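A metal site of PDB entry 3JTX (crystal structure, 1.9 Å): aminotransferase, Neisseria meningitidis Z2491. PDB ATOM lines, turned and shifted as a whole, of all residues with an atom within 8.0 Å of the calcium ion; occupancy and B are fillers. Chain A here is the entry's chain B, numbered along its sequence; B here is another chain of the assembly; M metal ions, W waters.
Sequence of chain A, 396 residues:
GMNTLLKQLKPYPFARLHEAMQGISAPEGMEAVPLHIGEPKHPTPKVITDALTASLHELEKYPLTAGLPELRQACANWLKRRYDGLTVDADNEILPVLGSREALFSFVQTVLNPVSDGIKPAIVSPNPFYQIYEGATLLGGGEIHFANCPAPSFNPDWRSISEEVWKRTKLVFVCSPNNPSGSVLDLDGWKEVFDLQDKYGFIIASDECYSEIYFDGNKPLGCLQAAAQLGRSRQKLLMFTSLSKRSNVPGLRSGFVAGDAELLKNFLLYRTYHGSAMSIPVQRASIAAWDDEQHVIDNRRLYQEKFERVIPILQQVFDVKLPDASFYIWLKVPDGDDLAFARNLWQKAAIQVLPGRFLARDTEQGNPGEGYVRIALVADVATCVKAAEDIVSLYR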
ATOM      1  N   SER A 106     -10.251  -7.682 -14.132  1.00  0.00           N
ATOM      2  CA  SER A 106     -10.662  -7.268 -15.481  1.00  0.00           C
ATOM      3  C   SER A 106     -11.817  -8.144 -16.013  1.00  0.00           C
ATOM      4  O   SER A 106     -12.779  -7.638 -16.639  1.00  0.00           O
ATOM      5  CB  SER A 106      -9.483  -7.260 -16.453  1.00  0.00           C
ATOM      6  OG  SER A 106      -8.850  -8.540 -16.589  1.00  0.00           O
ATOM      7  N   PHE A 107     -11.748  -9.453 -15.781  1.00  0.00           N
ATOM      8  CA  PHE A 107     -12.854 -10.318 -16.238  1.00  0.00           C
ATOM      9  C   PHE A 107     -14.174  -9.880 -15.606  1.00  0.00           C
ATOM     10  O   PHE A 107     -15.168  -9.712 -16.292  1.00  0.00           O
ATOM     11  CB  PHE A 107     -12.604 -11.791 -15.938  1.00  0.00           C
ATOM     12  CG  PHE A 107     -13.609 -12.665 -16.617  1.00  0.00           C
ATOM     13  CD1 PHE A 107     -13.617 -12.771 -17.996  1.00  0.00           C
ATOM     14  CD2 PHE A 107     -14.629 -13.280 -15.897  1.00  0.00           C
ATOM     15  CE1 PHE A 107     -14.610 -13.503 -18.655  1.00  0.00           C
ATOM     16  CE2 PHE A 107     -15.588 -14.031 -16.540  1.00  0.00           C
ATOM     17  CZ  PHE A 107     -15.574 -14.144 -17.916  1.00  0.00           C
ATOM     18  N   VAL A 108     -14.155  -9.632 -14.294  1.00  0.00           N
ATOM     19  CA  VAL A 108     -15.355  -9.140 -13.625  1.00  0.00           C
ATOM     20  C   VAL A 108     -15.899  -7.849 -14.261  1.00  0.00           C
ATOM     21  O   VAL A 108     -17.131  -7.718 -14.465  1.00  0.00           O
ATOM     22  CB  VAL A 108     -15.114  -8.966 -12.122  1.00  0.00           C
ATOM     23  CG1 VAL A 108     -16.250  -8.133 -11.474  1.00  0.00           C
ATOM     24  CG2 VAL A 108     -14.999 -10.323 -11.467  1.00  0.00           C
ATOM     25  N   GLN A 109     -15.000  -6.906 -14.573  1.00  0.00           N
ATOM     26  CA  GLN A 109     -15.409  -5.641 -15.216  1.00  0.00           C
ATOM     27  C   GLN A 109     -16.175  -5.946 -16.507  1.00  0.00           C
ATOM     28  O   GLN A 109     -17.150  -5.274 -16.801  1.00  0.00           O
ATOM     29  CB  GLN A 109     -14.243  -4.701 -15.526  1.00  0.00           C
ATOM     30  CG  GLN A 109     -13.378  -4.296 -14.318  1.00  0.00           C
ATOM     31  CD  GLN A 109     -14.202  -4.028 -13.077  1.00  0.00           C
ATOM     32  OE1 GLN A 109     -14.908  -3.008 -13.009  1.00  0.00           O
ATOM     33  NE2 GLN A 109     -14.139  -4.951 -12.105  1.00  0.00           N
ATOM     34  N   THR A 110     -15.746  -6.945 -17.274  1.00  0.00           N
ATOM     35  CA  THR A 110     -16.434  -7.260 -18.538  1.00  0.00           C
ATOM     36  C   THR A 110     -17.790  -7.950 -18.314  1.00  0.00           C
ATOM     37  O   THR A 110     -18.685  -7.814 -19.137  1.00  0.00           O
ATOM     38  CB  THR A 110     -15.562  -8.122 -19.471  1.00  0.00           C
ATOM     39  OG1 THR A 110     -15.496  -9.467 -18.975  1.00  0.00           O
ATOM     40  CG2 THR A 110     -14.127  -7.534 -19.604  1.00  0.00           C
ATOM     41  N   VAL A 111     -17.938  -8.664 -17.211  1.00  0.00           N
ATOM     42  CA  VAL A 111     -19.154  -9.427 -16.907  1.00  0.00           C
ATOM     43  C   VAL A 111     -20.248  -8.485 -16.381  1.00  0.00           C
ATOM     44  O   VAL A 111     -21.430  -8.704 -16.627  1.00  0.00           O
ATOM     45  CB  VAL A 111     -18.837 -10.575 -15.884  1.00  0.00           C
ATOM     46  CG1 VAL A 111     -20.094 -11.204 -15.339  1.00  0.00           C
ATOM     47  CG2 VAL A 111     -17.952 -11.611 -16.522  1.00  0.00           C
ATOM     48  N   LEU A 112     -19.865  -7.461 -15.631  1.00  0.00           N
ATOM     49  CA  LEU A 112     -20.840  -6.558 -15.003  1.00  0.00           C
ATOM     50  C   LEU A 112     -21.045  -5.336 -15.866  1.00  0.00           C
ATOM     51  O   LEU A 112     -20.111  -4.581 -16.100  1.00  0.00           O
ATOM     52  CB  LEU A 112     -20.358  -6.137 -13.623  1.00  0.00           C
ATOM     53  CG  LEU A 112     -20.272  -7.249 -12.593  1.00  0.00           C
ATOM     54  CD1 LEU A 112     -19.610  -6.719 -11.325  1.00  0.00           C
ATOM     55  CD2 LEU A 112     -21.688  -7.806 -12.300  1.00  0.00           C
ATOM     56  N   ASN A 113     -22.278  -5.143 -16.321  1.00  0.00           N
ATOM     57  CA  ASN A 113     -22.635  -4.026 -17.205  1.00  0.00           C
ATOM     58  C   ASN A 113     -24.002  -3.481 -16.834  1.00  0.00           C
ATOM     59  O   ASN A 113     -24.965  -3.620 -17.594  1.00  0.00           O
ATOM     60  CB  ASN A 113     -22.610  -4.487 -18.673  1.00  0.00           C
ATOM     61  CG  ASN A 113     -21.243  -5.052 -19.085  1.00  0.00           C
ATOM     62  OD1 ASN A 113     -20.210  -4.437 -18.838  1.00  0.00           O
ATOM     63  ND2 ASN A 113     -21.252  -6.240 -19.675  1.00  0.00           N
ATOM     64  N   PRO A 114     -24.106  -2.872 -15.641  1.00  0.00           N
ATOM     65  CA  PRO A 114     -25.381  -2.343 -15.157  1.00  0.00           C
ATOM     66  C   PRO A 114     -25.852  -1.172 -16.022  1.00  0.00           C
ATOM     67  O   PRO A 114     -25.015  -0.559 -16.689  1.00  0.00           O
ATOM     68  CB  PRO A 114     -25.066  -1.897 -13.726  1.00  0.00           C
ATOM     69  CG  PRO A 114     -23.640  -1.551 -13.748  1.00  0.00           C
ATOM     70  CD  PRO A 114     -22.980  -2.431 -14.788  1.00  0.00           C
ATOM     71  N   LEU A 139     -16.428  -2.231  -7.761  1.00  0.00           N
ATOM     72  CA  LEU A 139     -15.930  -1.276  -8.756  1.00  0.00           C
ATOM     73  C   LEU A 139     -16.506  -1.524 -10.131  1.00  0.00           C
ATOM     74  O   LEU A 139     -16.532  -0.621 -10.947  1.00  0.00           O
ATOM     75  CB  LEU A 139     -14.391  -1.272  -8.786  1.00  0.00           C
ATOM     76  CG  LEU A 139     -13.749  -0.744  -7.505  1.00  0.00           C
ATOM     77  CD1 LEU A 139     -12.245  -0.941  -7.519  1.00  0.00           C
ATOM     78  CD2 LEU A 139     -14.093   0.723  -7.311  1.00  0.00           C
ATOM     79  N   GLY A 140     -16.983  -2.730 -10.398  1.00  0.00           N
ATOM     80  CA  GLY A 140     -17.686  -3.034 -11.638  1.00  0.00           C
ATOM     81  C   GLY A 140     -19.158  -2.681 -11.647  1.00  0.00           C
ATOM     82  O   GLY A 140     -19.830  -2.907 -12.641  1.00  0.00           O
ATOM     83  N   GLY A 141     -19.652  -2.123 -10.542  1.00  0.00           N
ATOM     84  CA  GLY A 141     -21.035  -1.703 -10.414  1.00  0.00           C
ATOM     85  C   GLY A 141     -21.988  -2.820  -9.997  1.00  0.00           C
ATOM     86  O   GLY A 141     -23.189  -2.689 -10.158  1.00  0.00           O
ATOM     87  N   TYR A 270     -10.844  -7.364 -25.190  1.00  0.00           N
ATOM     88  CA  TYR A 270     -10.824  -6.362 -24.128  1.00  0.00           C
ATOM     89  C   TYR A 270      -9.400  -6.100 -23.616  1.00  0.00           C
ATOM     90  O   TYR A 270      -8.966  -4.963 -23.483  1.00  0.00           O
ATOM     91  CB  TYR A 270     -11.692  -6.819 -22.961  1.00  0.00           C
ATOM     92  CG  TYR A 270     -11.774  -5.869 -21.801  1.00  0.00           C
ATOM     93  CD1 TYR A 270     -12.693  -4.835 -21.793  1.00  0.00           C
ATOM     94  CD2 TYR A 270     -10.955  -6.022 -20.691  1.00  0.00           C
ATOM     95  CE1 TYR A 270     -12.798  -3.963 -20.726  1.00  0.00           C
ATOM     96  CE2 TYR A 270     -11.062  -5.145 -19.602  1.00  0.00           C
ATOM     97  CZ  TYR A 270     -11.989  -4.129 -19.642  1.00  0.00           C
ATOM     98  OH  TYR A 270     -12.127  -3.259 -18.581  1.00  0.00           O
ATOM     99  N   MET B   2     -21.178  -4.665 -24.743  1.00  0.00           N
ATOM    100  CA  MET B   2     -19.755  -5.028 -24.611  1.00  0.00           C
ATOM    101  C   MET B   2     -19.187  -5.750 -25.849  1.00  0.00           C
ATOM    102  O   MET B   2     -18.312  -5.250 -26.532  1.00  0.00           O
ATOM    103  CB  MET B   2     -19.594  -5.910 -23.360  1.00  0.00           C
ATOM    104  CG  MET B   2     -18.171  -6.432 -23.072  1.00  0.00           C
ATOM    105  SD  MET B   2     -16.904  -5.125 -22.284  1.00  0.00           S
ATOM    106  CE  MET B   2     -15.338  -6.264 -22.316  1.00  0.00           C
ATOM    107  N   GLN B 109     -11.238   4.619 -17.180  1.00  0.00           N
ATOM    108  CA  GLN B 109     -12.357   3.873 -16.563  1.00  0.00           C
ATOM    109  C   GLN B 109     -12.794   4.536 -15.245  1.00  0.00           C
ATOM    110  O   GLN B 109     -14.007   4.656 -14.997  1.00  0.00           O
ATOM    111  CB  GLN B 109     -12.031   2.398 -16.303  1.00  0.00           C
ATOM    112  CG  GLN B 109     -11.563   1.599 -17.507  1.00  0.00           C
ATOM    113  CD  GLN B 109     -12.348   1.878 -18.774  1.00  0.00           C
ATOM    114  OE1 GLN B 109     -13.527   1.516 -18.883  1.00  0.00           O
ATOM    115  NE2 GLN B 109     -11.699   2.516 -19.753  1.00  0.00           N
ATOM    116  N   LEU B 139     -15.259   1.788 -24.146  1.00  0.00           N
ATOM    117  CA  LEU B 139     -15.407   0.698 -23.179  1.00  0.00           C
ATOM    118  C   LEU B 139     -15.764   1.210 -21.785  1.00  0.00           C
ATOM    119  O   LEU B 139     -16.419   0.490 -21.036  1.00  0.00           O
ATOM    120  CB  LEU B 139     -14.173  -0.203 -23.128  1.00  0.00           C
ATOM    121  CG  LEU B 139     -13.985  -1.041 -24.397  1.00  0.00           C
ATOM    122  CD1 LEU B 139     -12.540  -1.538 -24.493  1.00  0.00           C
ATOM    123  CD2 LEU B 139     -15.003  -2.207 -24.436  1.00  0.00           C
ATOM    124  N   GLY B 140     -15.387   2.436 -21.438  1.00  0.00           N
ATOM    125  CA  GLY B 140     -15.808   3.056 -20.191  1.00  0.00           C
ATOM    126  C   GLY B 140     -17.208   3.663 -20.166  1.00  0.00           C
ATOM    127  O   GLY B 140     -17.614   4.236 -19.151  1.00  0.00           O
HETATM  128 CA    CA M   1     -18.470  -3.341 -17.187  1.00  0.00          CA
HETATM  129  O   HOH W   1     -18.508  -2.730 -15.032  1.00  0.00           O
HETATM  130  O   HOH W   2     -17.531  -3.524 -19.256  1.00  0.00           O
HETATM  131  O   HOH W   3     -16.590  -1.852 -17.016  1.00  0.00           O
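The backbone NH (N) of Gly 140 of chain A lies close to the side-chain amide oxygen (OE1) of Gln 109 of chain A (3.3 Å).
ND2 of Asn 113 is in hydrogen-bond range of O of Thr 110, at 3.1 Å.
The calcium ion is bound by water W1 (2.2 Å).
The calcium ion is bound by water W2 (2.3 Å).
The calcium ion is bound by O of Leu 112 (2.3 Å).
The calcium ion is bound by O of Gln 109 of chain A, 2.4 Å away.
The calcium ion is bound by water W3.
The calcium ion is bound by the side-chain amide oxygen (OD1) of Asn 113.
The calcium ion has six donor atoms within binding distance.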
